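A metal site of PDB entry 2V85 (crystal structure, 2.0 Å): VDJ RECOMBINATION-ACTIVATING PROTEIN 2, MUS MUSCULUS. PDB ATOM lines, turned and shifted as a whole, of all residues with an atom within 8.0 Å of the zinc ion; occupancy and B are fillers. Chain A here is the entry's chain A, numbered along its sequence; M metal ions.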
ATOM      1  N   CYS A  14     -14.559 -14.436 -15.136  1.00  0.00           N
ATOM      2  CA  CYS A  14     -13.752 -14.236 -13.936  1.00  0.00           C
ATOM      3  C   CYS A  14     -12.274 -13.925 -14.090  1.00  0.00           C
ATOM      4  O   CYS A  14     -11.693 -13.283 -13.229  1.00  0.00           O
ATOM      5  CB  CYS A  14     -13.917 -15.425 -12.985  1.00  0.00           C
ATOM      6  SG  CYS A  14     -12.967 -16.906 -13.407  1.00  0.00           S
ATOM      7  N   CYS A  15     -11.657 -14.401 -15.165  1.00  0.00           N
ATOM      8  CA  CYS A  15     -10.226 -14.160 -15.373  1.00  0.00           C
ATOM      9  C   CYS A  15      -9.887 -14.318 -16.850  1.00  0.00           C
ATOM     10  O   CYS A  15     -10.676 -14.820 -17.623  1.00  0.00           O
ATOM     11  CB  CYS A  15      -9.410 -15.145 -14.528  1.00  0.00           C
ATOM     12  SG  CYS A  15      -9.609 -16.863 -15.035  1.00  0.00           S
ATOM     13  N   ILE A  39     -15.527 -18.742  -5.626  1.00  0.00           N
ATOM     14  CA  ILE A  39     -14.782 -18.393  -4.418  1.00  0.00           C
ATOM     15  C   ILE A  39     -14.300 -16.951  -4.559  1.00  0.00           C
ATOM     16  O   ILE A  39     -13.916 -16.513  -5.629  1.00  0.00           O
ATOM     17  CB  ILE A  39     -13.577 -19.335  -4.195  1.00  0.00           C
ATOM     18  CG1 ILE A  39     -12.963 -19.105  -2.799  1.00  0.00           C
ATOM     19  CG2 ILE A  39     -12.578 -19.176  -5.315  1.00  0.00           C
ATOM     20  CD1 ILE A  39     -12.205 -17.805  -2.631  1.00  0.00           C
ATOM     21  N   TYR A  40     -14.299 -16.234  -3.447  1.00  0.00           N
ATOM     22  CA  TYR A  40     -13.864 -14.845  -3.431  1.00  0.00           C
ATOM     23  C   TYR A  40     -12.358 -14.682  -3.288  1.00  0.00           C
ATOM     24  O   TYR A  40     -11.748 -15.271  -2.409  1.00  0.00           O
ATOM     25  CB  TYR A  40     -14.570 -14.100  -2.288  1.00  0.00           C
ATOM     26  CG  TYR A  40     -14.619 -12.598  -2.434  1.00  0.00           C
ATOM     27  CD1 TYR A  40     -15.439 -12.010  -3.397  1.00  0.00           C
ATOM     28  CD2 TYR A  40     -13.852 -11.758  -1.620  1.00  0.00           C
ATOM     29  CE1 TYR A  40     -15.500 -10.619  -3.538  1.00  0.00           C
ATOM     30  CE2 TYR A  40     -13.904 -10.365  -1.756  1.00  0.00           C
ATOM     31  CZ  TYR A  40     -14.736  -9.812  -2.725  1.00  0.00           C
ATOM     32  OH  TYR A  40     -14.813  -8.443  -2.892  1.00  0.00           O
ATOM     33  N   CYS A  41     -11.767 -13.869  -4.154  1.00  0.00           N
ATOM     34  CA  CYS A  41     -10.343 -13.580  -4.087  1.00  0.00           C
ATOM     35  C   CYS A  41     -10.262 -12.312  -3.242  1.00  0.00           C
ATOM     36  O   CYS A  41     -10.934 -11.332  -3.530  1.00  0.00           O
ATOM     37  CB  CYS A  41      -9.766 -13.292  -5.472  1.00  0.00           C
ATOM     38  SG  CYS A  41      -8.107 -12.585  -5.405  1.00  0.00           S
ATOM     39  N   SER A  42      -9.432 -12.344  -2.199  1.00  0.00           N
ATOM     40  CA  SER A  42      -9.318 -11.214  -1.290  1.00  0.00           C
ATOM     41  C   SER A  42      -8.355 -10.103  -1.685  1.00  0.00           C
ATOM     42  O   SER A  42      -8.096  -9.202  -0.899  1.00  0.00           O
ATOM     43  CB  SER A  42      -8.962 -11.721   0.117  1.00  0.00           C
ATOM     44  OG  SER A  42      -9.986 -12.553   0.631  1.00  0.00           O
ATOM     45  N   HIS A  43      -7.821 -10.156  -2.901  1.00  0.00           N
ATOM     46  CA  HIS A  43      -6.894  -9.104  -3.331  1.00  0.00           C
ATOM     47  C   HIS A  43      -7.582  -7.753  -3.451  1.00  0.00           C
ATOM     48  O   HIS A  43      -8.563  -7.611  -4.173  1.00  0.00           O
ATOM     49  CB  HIS A  43      -6.266  -9.467  -4.673  1.00  0.00           C
ATOM     50  CG  HIS A  43      -5.387  -8.389  -5.220  1.00  0.00           C
ATOM     51  ND1 HIS A  43      -4.164  -8.079  -4.677  1.00  0.00           N
ATOM     52  CD2 HIS A  43      -5.592  -7.505  -6.232  1.00  0.00           C
ATOM     53  CE1 HIS A  43      -3.644  -7.048  -5.334  1.00  0.00           C
ATOM     54  NE2 HIS A  43      -4.490  -6.685  -6.278  1.00  0.00           N
ATOM     55  N   GLY A  44      -7.062  -6.741  -2.751  1.00  0.00           N
ATOM     56  CA  GLY A  44      -7.663  -5.415  -2.804  1.00  0.00           C
ATOM     57  C   GLY A  44      -9.086  -5.469  -2.303  1.00  0.00           C
ATOM     58  O   GLY A  44      -9.341  -6.071  -1.272  1.00  0.00           O
ATOM     59  N   GLY A  46     -11.261  -7.070  -3.568  1.00  0.00           N
ATOM     60  CA  GLY A  46     -11.689  -8.437  -3.825  1.00  0.00           C
ATOM     61  C   GLY A  46     -12.570  -8.638  -5.036  1.00  0.00           C
ATOM     62  O   GLY A  46     -13.085  -7.686  -5.605  1.00  0.00           O
ATOM     63  N   HIS A  47     -12.727  -9.890  -5.441  1.00  0.00           N
ATOM     64  CA  HIS A  47     -13.560 -10.216  -6.578  1.00  0.00           C
ATOM     65  C   HIS A  47     -13.865 -11.714  -6.638  1.00  0.00           C
ATOM     66  O   HIS A  47     -13.089 -12.524  -6.144  1.00  0.00           O
ATOM     67  CB  HIS A  47     -12.874  -9.767  -7.873  1.00  0.00           C
ATOM     68  CG  HIS A  47     -11.584 -10.455  -8.159  1.00  0.00           C
ATOM     69  ND1 HIS A  47     -11.450 -11.403  -9.159  1.00  0.00           N
ATOM     70  CD2 HIS A  47     -10.367 -10.345  -7.581  1.00  0.00           C
ATOM     71  CE1 HIS A  47     -10.206 -11.840  -9.191  1.00  0.00           C
ATOM     72  NE2 HIS A  47      -9.519 -11.211  -8.240  1.00  0.00           N
ATOM     73  N   TRP A  48     -14.999 -12.064  -7.222  1.00  0.00           N
ATOM     74  CA  TRP A  48     -15.411 -13.459  -7.343  1.00  0.00           C
ATOM     75  C   TRP A  48     -14.846 -14.127  -8.583  1.00  0.00           C
ATOM     76  O   TRP A  48     -14.808 -13.536  -9.658  1.00  0.00           O
ATOM     77  CB  TRP A  48     -16.936 -13.571  -7.387  1.00  0.00           C
ATOM     78  CG  TRP A  48     -17.627 -13.270  -6.116  1.00  0.00           C
ATOM     79  CD1 TRP A  48     -18.158 -12.072  -5.721  1.00  0.00           C
ATOM     80  CD2 TRP A  48     -17.869 -14.186  -5.033  1.00  0.00           C
ATOM     81  NE1 TRP A  48     -18.727 -12.186  -4.472  1.00  0.00           N
ATOM     82  CE2 TRP A  48     -18.564 -13.467  -4.030  1.00  0.00           C
ATOM     83  CE3 TRP A  48     -17.575 -15.532  -4.828  1.00  0.00           C
ATOM     84  CZ2 TRP A  48     -18.949 -14.068  -2.819  1.00  0.00           C
ATOM     85  CZ3 TRP A  48     -17.957 -16.131  -3.626  1.00  0.00           C
ATOM     86  CH2 TRP A  48     -18.643 -15.394  -2.648  1.00  0.00           C
ATOM     87  N   VAL A  49     -14.422 -15.380  -8.426  1.00  0.00           N
ATOM     88  CA  VAL A  49     -13.904 -16.170  -9.544  1.00  0.00           C
ATOM     89  C   VAL A  49     -14.558 -17.560  -9.476  1.00  0.00           C
ATOM     90  O   VAL A  49     -15.054 -17.956  -8.432  1.00  0.00           O
ATOM     91  CB  VAL A  49     -12.363 -16.354  -9.484  1.00  0.00           C
ATOM     92  CG1 VAL A  49     -11.661 -15.017  -9.708  1.00  0.00           C
ATOM     93  CG2 VAL A  49     -11.960 -16.970  -8.160  1.00  0.00           C
ATOM     94  N   MET A  54      -9.762 -21.810 -11.485  1.00  0.00           N
ATOM     95  CA  MET A  54      -8.551 -21.710 -10.672  1.00  0.00           C
ATOM     96  C   MET A  54      -7.867 -23.067 -10.522  1.00  0.00           C
ATOM     97  O   MET A  54      -6.862 -23.191  -9.852  1.00  0.00           O
ATOM     98  CB  MET A  54      -8.911 -21.193  -9.273  1.00  0.00           C
ATOM     99  CG  MET A  54      -9.708 -19.918  -9.283  1.00  0.00           C
ATOM    100  SD  MET A  54      -8.639 -18.472  -9.373  1.00  0.00           S
ATOM    101  CE  MET A  54      -8.512 -18.237 -10.935  1.00  0.00           C
ATOM    102  N   TYR A  71      -8.642 -16.508   0.338  1.00  0.00           N
ATOM    103  CA  TYR A  71      -8.164 -17.110  -0.898  1.00  0.00           C
ATOM    104  C   TYR A  71      -7.716 -15.999  -1.847  1.00  0.00           C
ATOM    105  O   TYR A  71      -8.290 -14.916  -1.864  1.00  0.00           O
ATOM    106  CB  TYR A  71      -9.268 -17.936  -1.563  1.00  0.00           C
ATOM    107  CG  TYR A  71      -8.870 -18.457  -2.924  1.00  0.00           C
ATOM    108  CD1 TYR A  71      -9.378 -17.891  -4.095  1.00  0.00           C
ATOM    109  CD2 TYR A  71      -7.905 -19.462  -3.047  1.00  0.00           C
ATOM    110  CE1 TYR A  71      -8.932 -18.307  -5.354  1.00  0.00           C
ATOM    111  CE2 TYR A  71      -7.454 -19.879  -4.293  1.00  0.00           C
ATOM    112  CZ  TYR A  71      -7.967 -19.297  -5.439  1.00  0.00           C
ATOM    113  OH  TYR A  71      -7.495 -19.665  -6.682  1.00  0.00           O
ATOM    114  N   TYR A  72      -6.676 -16.291  -2.624  1.00  0.00           N
ATOM    115  CA  TYR A  72      -6.162 -15.334  -3.605  1.00  0.00           C
ATOM    116  C   TYR A  72      -6.046 -16.049  -4.938  1.00  0.00           C
ATOM    117  O   TYR A  72      -5.397 -17.076  -5.042  1.00  0.00           O
ATOM    118  CB  TYR A  72      -4.797 -14.790  -3.151  1.00  0.00           C
ATOM    119  CG  TYR A  72      -4.901 -13.951  -1.898  1.00  0.00           C
ATOM    120  CD1 TYR A  72      -4.764 -14.527  -0.636  1.00  0.00           C
ATOM    121  CD2 TYR A  72      -5.187 -12.593  -1.970  1.00  0.00           C
ATOM    122  CE1 TYR A  72      -4.914 -13.772   0.524  1.00  0.00           C
ATOM    123  CE2 TYR A  72      -5.343 -11.819  -0.807  1.00  0.00           C
ATOM    124  CZ  TYR A  72      -5.210 -12.425   0.433  1.00  0.00           C
ATOM    125  OH  TYR A  72      -5.350 -11.686   1.580  1.00  0.00           O
ATOM    126  N   CYS A  73      -6.696 -15.501  -5.963  1.00  0.00           N
ATOM    127  CA  CYS A  73      -6.692 -16.117  -7.282  1.00  0.00           C
ATOM    128  C   CYS A  73      -5.291 -16.204  -7.873  1.00  0.00           C
ATOM    129  O   CYS A  73      -4.369 -15.540  -7.423  1.00  0.00           O
ATOM    130  CB  CYS A  73      -7.613 -15.350  -8.245  1.00  0.00           C
ATOM    131  SG  CYS A  73      -6.936 -13.819  -8.898  1.00  0.00           S
ATOM    132  N   ASN A  74      -5.156 -17.055  -8.875  1.00  0.00           N
ATOM    133  CA  ASN A  74      -3.880 -17.301  -9.530  1.00  0.00           C
ATOM    134  C   ASN A  74      -3.236 -16.020 -10.095  1.00  0.00           C
ATOM    135  O   ASN A  74      -2.032 -15.928 -10.181  1.00  0.00           O
ATOM    136  CB  ASN A  74      -4.072 -18.383 -10.618  1.00  0.00           C
ATOM    137  CG  ASN A  74      -4.448 -19.752 -10.016  1.00  0.00           C
ATOM    138  OD1 ASN A  74      -4.845 -20.679 -10.724  1.00  0.00           O
ATOM    139  ND2 ASN A  74      -4.317 -19.880  -8.704  1.00  0.00           N
ATOM    140  N   GLU A  75      -4.052 -15.028 -10.423  1.00  0.00           N
ATOM    141  CA  GLU A  75      -3.558 -13.751 -10.944  1.00  0.00           C
ATOM    142  C   GLU A  75      -2.971 -12.811  -9.881  1.00  0.00           C
ATOM    143  O   GLU A  75      -2.115 -11.997 -10.180  1.00  0.00           O
ATOM    144  CB  GLU A  75      -4.671 -13.003 -11.668  1.00  0.00           C
ATOM    145  CG  GLU A  75      -4.869 -13.353 -13.119  1.00  0.00           C
ATOM    146  CD  GLU A  75      -5.936 -12.504 -13.779  1.00  0.00           C
ATOM    147  OE1 GLU A  75      -7.138 -12.784 -13.592  1.00  0.00           O
ATOM    148  OE2 GLU A  75      -5.575 -11.529 -14.480  1.00  0.00           O
ATOM    149  N   HIS A  76      -3.453 -12.915  -8.646  1.00  0.00           N
ATOM    150  CA  HIS A  76      -3.018 -12.014  -7.585  1.00  0.00           C
ATOM    151  C   HIS A  76      -2.261 -12.666  -6.431  1.00  0.00           C
ATOM    152  O   HIS A  76      -1.737 -11.979  -5.570  1.00  0.00           O
ATOM    153  CB  HIS A  76      -4.250 -11.305  -7.003  1.00  0.00           C
ATOM    154  CG  HIS A  76      -4.975 -10.447  -7.984  1.00  0.00           C
ATOM    155  ND1 HIS A  76      -6.347 -10.443  -8.105  1.00  0.00           N
ATOM    156  CD2 HIS A  76      -4.511  -9.542  -8.890  1.00  0.00           C
ATOM    157  CE1 HIS A  76      -6.703  -9.578  -9.042  1.00  0.00           C
ATOM    158  NE2 HIS A  76      -5.606  -9.015  -9.529  1.00  0.00           N
ATOM    159  N   VAL A  77      -2.208 -13.984  -6.418  1.00  0.00           N
ATOM    160  CA  VAL A  77      -1.556 -14.712  -5.336  1.00  0.00           C
ATOM    161  C   VAL A  77      -0.081 -14.379  -5.060  1.00  0.00           C
ATOM    162  O   VAL A  77       0.346 -14.463  -3.931  1.00  0.00           O
ATOM    163  CB  VAL A  77      -1.739 -16.229  -5.552  1.00  0.00           C
ATOM    164  CG1 VAL A  77      -0.847 -16.723  -6.679  1.00  0.00           C
ATOM    165  CG2 VAL A  77      -1.473 -16.970  -4.261  1.00  0.00           C
ATOM    166  N   ILE A  79       1.301 -11.418  -5.482  1.00  0.00           N
ATOM    167  CA  ILE A  79       1.458 -10.023  -5.099  1.00  0.00           C
ATOM    168  C   ILE A  79       1.758  -9.932  -3.617  1.00  0.00           C
ATOM    169  O   ILE A  79       1.084 -10.530  -2.799  1.00  0.00           O
ATOM    170  CB  ILE A  79       0.208  -9.210  -5.465  1.00  0.00           C
ATOM    171  CG1 ILE A  79      -0.066  -9.321  -6.965  1.00  0.00           C
ATOM    172  CG2 ILE A  79       0.405  -7.750  -5.077  1.00  0.00           C
ATOM    173  CD1 ILE A  79      -1.283  -8.573  -7.451  1.00  0.00           C
HETATM  174 ZN    ZN M   1      -7.747 -12.086  -7.565  1.00  0.00          ZN
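Four residues have an atom within 4 Å of the zinc ion: Cys 41, His 47, Cys 73 and His 76.
The nearest printed residue that does not touch the zinc ion is His 43 (4.2 Å).
The zinc ion is bound by a ring nitrogen (NE2) of His 47 (2.1 Å), a ring nitrogen (ND1) of His 76 (2.2 Å), the side-chain sulfur (SG) of Cys 41 (2.2 Å) and the side-chain sulfur (SG) of Cys 73 (2.3 Å).
The side-chain sulfur (SG) of Cys 73 lies close to the backbone NH (N) of Glu 75 (3.5 Å).
SG of Cys 41 lies close to N of His 43 (3.5 Å).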
